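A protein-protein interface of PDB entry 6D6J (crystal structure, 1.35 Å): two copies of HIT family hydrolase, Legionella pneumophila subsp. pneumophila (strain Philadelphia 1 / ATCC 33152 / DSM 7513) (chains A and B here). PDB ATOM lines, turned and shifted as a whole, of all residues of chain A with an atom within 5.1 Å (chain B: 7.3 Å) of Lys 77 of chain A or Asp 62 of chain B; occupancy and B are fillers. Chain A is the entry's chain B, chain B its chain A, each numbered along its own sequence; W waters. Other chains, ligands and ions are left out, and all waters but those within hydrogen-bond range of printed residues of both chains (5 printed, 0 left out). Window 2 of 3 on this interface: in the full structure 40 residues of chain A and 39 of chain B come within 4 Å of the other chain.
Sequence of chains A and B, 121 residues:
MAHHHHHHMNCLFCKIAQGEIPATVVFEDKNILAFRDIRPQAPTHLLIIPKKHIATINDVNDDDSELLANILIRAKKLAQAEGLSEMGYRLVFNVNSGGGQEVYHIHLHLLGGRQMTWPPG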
ATOM      1  N   ASN A  70      15.613 -16.060   5.502  1.00  0.00           N
ATOM      2  CA  ASN A  70      16.058 -17.352   6.009  1.00  0.00           C
ATOM      3  C   ASN A  70      17.518 -17.619   5.675  1.00  0.00           C
ATOM      4  O   ASN A  70      18.204 -18.323   6.428  1.00  0.00           O
ATOM      5  CB  ASN A  70      15.136 -18.461   5.510  1.00  0.00           C
ATOM      6  CG  ASN A  70      13.820 -18.471   6.251  1.00  0.00           C
ATOM      7  OD1 ASN A  70      13.712 -17.901   7.341  1.00  0.00           O
ATOM      8  ND2 ASN A  70      12.819 -19.078   5.661  1.00  0.00           N
ATOM      9  N   ILE A  73      19.116 -15.797   8.545  1.00  0.00           N
ATOM     10  CA  ILE A  73      18.995 -16.589   9.763  1.00  0.00           C
ATOM     11  C   ILE A  73      19.941 -17.782   9.721  1.00  0.00           C
ATOM     12  O   ILE A  73      20.616 -18.085  10.710  1.00  0.00           O
ATOM     13  CB  ILE A  73      17.531 -17.003   9.979  1.00  0.00           C
ATOM     14  CG1 ILE A  73      16.667 -15.770  10.277  1.00  0.00           C
ATOM     15  CG2 ILE A  73      17.417 -18.015  11.128  1.00  0.00           C
ATOM     16  CD1 ILE A  73      15.177 -16.006  10.084  1.00  0.00           C
ATOM     17  N   ARG A  74      20.024 -18.469   8.579  1.00  0.00           N
ATOM     18  CA  ARG A  74      20.953 -19.587   8.488  1.00  0.00           C
ATOM     19  C   ARG A  74      22.391 -19.118   8.669  1.00  0.00           C
ATOM     20  O   ARG A  74      23.186 -19.797   9.334  1.00  0.00           O
ATOM     21  CB  ARG A  74      20.771 -20.342   7.175  1.00  0.00           C
ATOM     22  CG  ARG A  74      21.776 -21.504   6.986  1.00  0.00           C
ATOM     23  CD  ARG A  74      21.809 -22.449   8.198  1.00  0.00           C
ATOM     24  NE  ARG A  74      20.474 -22.933   8.550  1.00  0.00           N
ATOM     25  CZ  ARG A  74      20.197 -23.699   9.600  1.00  0.00           C
ATOM     26  NH1 ARG A  74      21.163 -24.037  10.452  1.00  0.00           N
ATOM     27  NH2 ARG A  74      18.944 -24.087   9.821  1.00  0.00           N
ATOM     28  N   ALA A  75      22.744 -17.948   8.118  1.00  0.00           N
ATOM     29  CA  ALA A  75      24.105 -17.450   8.318  1.00  0.00           C
ATOM     30  C   ALA A  75      24.440 -17.253   9.793  1.00  0.00           C
ATOM     31  O   ALA A  75      25.554 -17.580  10.224  1.00  0.00           O
ATOM     32  CB  ALA A  75      24.327 -16.155   7.555  1.00  0.00           C
ATOM     33  N   LYS A  76      23.494 -16.744  10.596  1.00  0.00           N
ATOM     34  CA  LYS A  76      23.783 -16.551  12.018  1.00  0.00           C
ATOM     35  C   LYS A  76      23.879 -17.876  12.764  1.00  0.00           C
ATOM     36  O   LYS A  76      24.660 -17.996  13.714  1.00  0.00           O
ATOM     37  CB  LYS A  76      22.847 -15.531  12.694  1.00  0.00           C
ATOM     38  CG  LYS A  76      21.381 -15.865  12.921  1.00  0.00           C
ATOM     39  CD  LYS A  76      21.093 -16.764  14.169  1.00  0.00           C
ATOM     40  CE  LYS A  76      21.616 -16.267  15.523  1.00  0.00           C
ATOM     41  NZ  LYS A  76      20.851 -16.925  16.647  1.00  0.00           N
ATOM     42  N   LYS A  77      23.109 -18.887  12.347  1.00  0.00           N
ATOM     43  CA  LYS A  77      23.248 -20.205  12.969  1.00  0.00           C
ATOM     44  C   LYS A  77      24.587 -20.820  12.590  1.00  0.00           C
ATOM     45  O   LYS A  77      25.287 -21.388  13.438  1.00  0.00           O
ATOM     46  CB  LYS A  77      22.086 -21.105  12.542  1.00  0.00           C
ATOM     47  CG  LYS A  77      20.731 -20.644  13.055  1.00  0.00           C
ATOM     48  CD  LYS A  77      19.597 -21.554  12.585  1.00  0.00           C
ATOM     49  CE  LYS A  77      18.282 -21.141  13.218  1.00  0.00           C
ATOM     50  NZ  LYS A  77      17.176 -22.008  12.756  1.00  0.00           N
ATOM     51  N   LEU A  78      24.964 -20.680  11.318  1.00  0.00           N
ATOM     52  CA  LEU A  78      26.215 -21.226  10.824  1.00  0.00           C
ATOM     53  C   LEU A  78      27.413 -20.557  11.483  1.00  0.00           C
ATOM     54  O   LEU A  78      28.415 -21.217  11.777  1.00  0.00           O
ATOM     55  CB  LEU A  78      26.232 -21.023   9.314  1.00  0.00           C
ATOM     56  CG  LEU A  78      27.437 -21.559   8.566  1.00  0.00           C
ATOM     57  CD1 LEU A  78      27.560 -23.092   8.734  1.00  0.00           C
ATOM     58  CD2 LEU A  78      27.302 -21.197   7.108  1.00  0.00           C
ATOM     59  N   ALA A  79      27.334 -19.240  11.717  1.00  0.00           N
ATOM     60  CA  ALA A  79      28.428 -18.546  12.398  1.00  0.00           C
ATOM     61  C   ALA A  79      28.682 -19.131  13.786  1.00  0.00           C
ATOM     62  O   ALA A  79      29.839 -19.220  14.231  1.00  0.00           O
ATOM     63  CB  ALA A  79      28.130 -17.051  12.495  1.00  0.00           C
ATOM     64  N   GLN A  80      27.618 -19.544  14.488  1.00  0.00           N
ATOM     65  CA  GLN A  80      27.798 -20.217  15.774  1.00  0.00           C
ATOM     66  C   GLN A  80      28.429 -21.593  15.586  1.00  0.00           C
ATOM     67  O   GLN A  80      29.369 -21.961  16.303  1.00  0.00           O
ATOM     68  CB  GLN A  80      26.442 -20.371  16.452  1.00  0.00           C
ATOM     69  CG  GLN A  80      25.829 -19.055  16.806  1.00  0.00           C
ATOM     70  CD  GLN A  80      24.430 -19.185  17.360  1.00  0.00           C
ATOM     71  OE1 GLN A  80      23.757 -20.205  17.171  1.00  0.00           O
ATOM     72  NE2 GLN A  80      23.967 -18.138  18.025  1.00  0.00           N
ATOM     73  N   ALA A  81      27.913 -22.376  14.631  1.00  0.00           N
ATOM     74  CA  ALA A  81      28.414 -23.731  14.412  1.00  0.00           C
ATOM     75  C   ALA A  81      29.885 -23.716  14.050  1.00  0.00           C
ATOM     76  O   ALA A  81      30.619 -24.649  14.394  1.00  0.00           O
ATOM     77  CB  ALA A  81      27.610 -24.403  13.297  1.00  0.00           C
ATOM     78  N   ILE B  57      22.840  -9.581  15.884  1.00  0.00           N
ATOM     79  CA  ILE B  57      22.387 -10.645  14.987  1.00  0.00           C
ATOM     80  C   ILE B  57      22.537 -12.013  15.642  1.00  0.00           C
ATOM     81  O   ILE B  57      21.788 -12.944  15.323  1.00  0.00           O
ATOM     82  CB  ILE B  57      23.109 -10.527  13.625  1.00  0.00           C
ATOM     83  CG1 ILE B  57      22.626  -9.271  12.886  1.00  0.00           C
ATOM     84  CG2 ILE B  57      22.954 -11.783  12.769  1.00  0.00           C
ATOM     85  CD1 ILE B  57      21.212  -9.350  12.327  1.00  0.00           C
ATOM     86  N   ASN B  58      23.472 -12.153  16.600  1.00  0.00           N
ATOM     87  CA  ASN B  58      23.643 -13.430  17.277  1.00  0.00           C
ATOM     88  C   ASN B  58      22.406 -13.822  18.082  1.00  0.00           C
ATOM     89  O   ASN B  58      22.266 -14.998  18.438  1.00  0.00           O
ATOM     90  CB  ASN B  58      24.875 -13.360  18.185  1.00  0.00           C
ATOM     91  CG  ASN B  58      25.434 -14.720  18.556  1.00  0.00           C
ATOM     92  OD1 ASN B  58      25.426 -15.651  17.756  1.00  0.00           O
ATOM     93  ND2 ASN B  58      25.943 -14.835  19.774  1.00  0.00           N
ATOM     94  N   ASP B  59      21.482 -12.886  18.331  1.00  0.00           N
ATOM     95  CA  ASP B  59      20.248 -13.143  19.069  1.00  0.00           C
ATOM     96  C   ASP B  59      19.061 -13.474  18.167  1.00  0.00           C
ATOM     97  O   ASP B  59      17.962 -13.733  18.677  1.00  0.00           O
ATOM     98  CB  ASP B  59      19.858 -11.899  19.885  1.00  0.00           C
ATOM     99  CG  ASP B  59      20.847 -11.557  20.980  1.00  0.00           C
ATOM    100  OD1 ASP B  59      21.580 -12.465  21.430  1.00  0.00           O
ATOM    101  OD2 ASP B  59      20.857 -10.372  21.398  1.00  0.00           O
ATOM    102  N   VAL B  60      19.231 -13.435  16.843  1.00  0.00           N
ATOM    103  CA  VAL B  60      18.110 -13.631  15.925  1.00  0.00           C
ATOM    104  C   VAL B  60      17.515 -15.030  16.056  1.00  0.00           C
ATOM    105  O   VAL B  60      18.221 -16.023  16.294  1.00  0.00           O
ATOM    106  CB  VAL B  60      18.610 -13.333  14.498  1.00  0.00           C
ATOM    107  CG1 VAL B  60      17.833 -14.111  13.426  1.00  0.00           C
ATOM    108  CG2 VAL B  60      18.615 -11.809  14.258  1.00  0.00           C
ATOM    109  N   ASN B  61      16.191 -15.108  15.891  1.00  0.00           N
ATOM    110  CA  ASN B  61      15.471 -16.380  15.905  1.00  0.00           C
ATOM    111  C   ASN B  61      14.609 -16.489  14.645  1.00  0.00           C
ATOM    112  O   ASN B  61      14.505 -15.550  13.839  1.00  0.00           O
ATOM    113  CB  ASN B  61      14.669 -16.572  17.210  1.00  0.00           C
ATOM    114  CG  ASN B  61      13.602 -15.500  17.415  1.00  0.00           C
ATOM    115  OD1 ASN B  61      13.020 -15.000  16.443  1.00  0.00           O
ATOM    116  ND2 ASN B  61      13.354 -15.127  18.669  1.00  0.00           N
ATOM    117  N   ASP B  62      13.985 -17.655  14.464  1.00  0.00           N
ATOM    118  CA  ASP B  62      13.192 -17.865  13.251  1.00  0.00           C
ATOM    119  C   ASP B  62      11.944 -17.001  13.222  1.00  0.00           C
ATOM    120  O   ASP B  62      11.453 -16.660  12.134  1.00  0.00           O
ATOM    121  CB  ASP B  62      12.875 -19.351  13.061  1.00  0.00           C
ATOM    122  CG  ASP B  62      14.095 -20.122  12.616  1.00  0.00           C
ATOM    123  OD1 ASP B  62      14.512 -19.936  11.454  1.00  0.00           O
ATOM    124  OD2 ASP B  62      14.667 -20.872  13.422  1.00  0.00           O
ATOM    125  N   ASP B  63      11.422 -16.617  14.387  1.00  0.00           N
ATOM    126  CA  ASP B  63      10.294 -15.691  14.408  1.00  0.00           C
ATOM    127  C   ASP B  63      10.668 -14.290  13.954  1.00  0.00           C
ATOM    128  O   ASP B  63       9.767 -13.498  13.704  1.00  0.00           O
ATOM    129  CB  ASP B  63       9.590 -15.698  15.769  1.00  0.00           C
ATOM    130  CG  ASP B  63       8.536 -16.793  15.874  1.00  0.00           C
ATOM    131  OD1 ASP B  63       7.949 -17.174  14.841  1.00  0.00           O
ATOM    132  OD2 ASP B  63       8.257 -17.251  16.995  1.00  0.00           O
ATOM    133  N   ASP B  64      11.959 -13.983  13.803  1.00  0.00           N
ATOM    134  CA  ASP B  64      12.373 -12.716  13.210  1.00  0.00           C
ATOM    135  C   ASP B  64      12.293 -12.702  11.689  1.00  0.00           C
ATOM    136  O   ASP B  64      12.603 -11.666  11.092  1.00  0.00           O
ATOM    137  CB  ASP B  64      13.829 -12.421  13.581  1.00  0.00           C
ATOM    138  CG  ASP B  64      14.014 -12.084  15.044  1.00  0.00           C
ATOM    139  OD1 ASP B  64      13.108 -11.482  15.669  1.00  0.00           O
ATOM    140  OD2 ASP B  64      15.098 -12.409  15.569  1.00  0.00           O
ATOM    141  N   SER B  65      11.919 -13.801  11.023  1.00  0.00           N
ATOM    142  CA  SER B  65      12.031 -13.813   9.566  1.00  0.00           C
ATOM    143  C   SER B  65      11.184 -12.723   8.914  1.00  0.00           C
ATOM    144  O   SER B  65      11.624 -12.095   7.944  1.00  0.00           O
ATOM    145  CB  SER B  65      11.718 -15.196   8.992  1.00  0.00           C
ATOM    146  OG  SER B  65      10.398 -15.603   9.296  1.00  0.00           O
ATOM    147  N   GLU B  66       9.982 -12.464   9.429  1.00  0.00           N
ATOM    148  CA  GLU B  66       9.153 -11.414   8.834  1.00  0.00           C
ATOM    149  C   GLU B  66       9.827 -10.047   8.933  1.00  0.00           C
ATOM    150  O   GLU B  66       9.900  -9.300   7.951  1.00  0.00           O
ATOM    151  CB  GLU B  66       7.781 -11.402   9.515  1.00  0.00           C
ATOM    152  CG  GLU B  66       6.848 -10.312   8.981  1.00  0.00           C
ATOM    153  CD  GLU B  66       5.448 -10.321   9.587  1.00  0.00           C
ATOM    154  OE1 GLU B  66       5.219 -11.027  10.587  1.00  0.00           O
ATOM    155  OE2 GLU B  66       4.583  -9.610   9.045  1.00  0.00           O
ATOM    156  N   LEU B  68      13.063  -9.370   9.460  1.00  0.00           N
ATOM    157  CA  LEU B  68      14.300  -9.324   8.692  1.00  0.00           C
ATOM    158  C   LEU B  68      14.023  -9.196   7.198  1.00  0.00           C
ATOM    159  O   LEU B  68      14.720  -8.456   6.494  1.00  0.00           O
ATOM    160  CB  LEU B  68      15.151 -10.544   8.990  1.00  0.00           C
ATOM    161  CG  LEU B  68      15.678 -10.608  10.431  1.00  0.00           C
ATOM    162  CD1 LEU B  68      16.341 -11.943  10.684  1.00  0.00           C
ATOM    163  CD2 LEU B  68      16.645  -9.466  10.744  1.00  0.00           C
HETATM  164  O   HOH W   1      16.368 -21.421  10.137  1.00  0.00           O
HETATM  165  O   HOH W   2      14.810 -23.858  11.812  1.00  0.00           O
HETATM  166  O   HOH W   3      12.699 -19.090   9.567  1.00  0.00           O
HETATM  167  O   HOH W   4      10.072 -18.627   7.718  1.00  0.00           O
HETATM  168  O   HOH W   5      25.640 -15.771  15.050  1.00  0.00           O
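NZ of Lys 76 of chain A is in hydrogen-bond range of O of Asn 58 of chain B (3.0 Å). OD1 of Asn 58 of chain B lies within hydrogen-bond range of NE2 of Gln 80 of chain A, 2.9 Å away. The backbone carbonyl oxygen (O) of Val 60 of chain B is in hydrogen-bond range of the side-chain amino group (NZ) of Lys 76 of chain A (2.8 Å). NZ of Lys 77 of chain A lies within salt-bridge range of OD2 of Asp 62 of chain B, 2.8 Å away.
The backbone NH (N) of Asp 63 of chain B lies within hydrogen-bond range of the side-chain amide oxygen (OD1) of Asn 61 of chain B, 3.1 Å away. N of Asn 61 of chain B lies within hydrogen-bond range of OD2 of Asp 64 of chain B. The side-chain hydroxyl (OG) of Ser 65 of chain B lies within hydrogen-bond range of the backbone carbonyl oxygen (O) of Asp 62 of chain B, 3.2 Å away.
Among the printed residues, merely in contact across the chains: Lys 76 of chain A with Ile 57 of chain B (3.3 Å), Ile 73 of chain A with Asp 62 of chain B (3.5 Å), Ile 73 of chain A with Ser 65 of chain B (3.7 Å), Asn 70 of chain A with Ser 65 of chain B (3.7 Å), Ile 73 of chain A with Val 60 of chain B (3.7 Å), Ile 73 of chain A with Asn 61 of chain B (3.8 Å) and Ile 73 of chain A with Leu 68 of chain B (3.9 Å).
Of chain B, only Asp 62 comes within 4 Å of Lys 77 of chain A. Of chain A, only Ile 73 (3.5 Å) and Lys 77 (2.8 Å) come within 4 Å of Asp 62 of chain B. Of the printed residues of chain A, Ser 65 of chain B touches Asn 70 (3.7 Å) and Ile 73 (3.7 Å). Of the printed residues of chain A, Leu 68 of chain B touches Ile 73 (3.9 Å). The nearest residue of chain B that does not touch Lys 77 of chain A is Val 60 of chain B (6.0 Å). The nearest printed residue of chain A that does not touch Leu 68 of chain B is Asn 70 of chain A (6.5 Å).
Hydrophobic or aromatic side chains of chain B that line the printed part of chain A: Ile 57, Val 60 and Leu 68. Hydrophobic or aromatic side chains of chain A within 4 Å of the printed part of chain B: Ile 73.
No position is printed for both chains.
Water W5 lies within hydrogen-bond range of the side-chain amide oxygen (OD1) of Asn 58 of chain B (2.7 Å) and the backbone carbonyl oxygen (O) of Lys 76 of chain A (2.8 Å). Water W1 lies within hydrogen-bond range of OD1 of Asp 62 of chain B (2.7 Å) and NZ of Lys 77 of chain A (2.8 Å). Water W3 bridges OD1 of Asn 70 of chain A (2.7 Å) and OD1 of Asp 62 of chain B (2.8 Å). Water W2 lies within hydrogen-bond range of NZ of Lys 77 of chain A (3.1 Å) and OD2 of Asp 62 of chain B (3.4 Å). Water W4 lies within hydrogen-bond range of OG of Ser 65 of chain B (3.4 Å) and ND2 of Asn 70 of chain A (3.5 Å).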
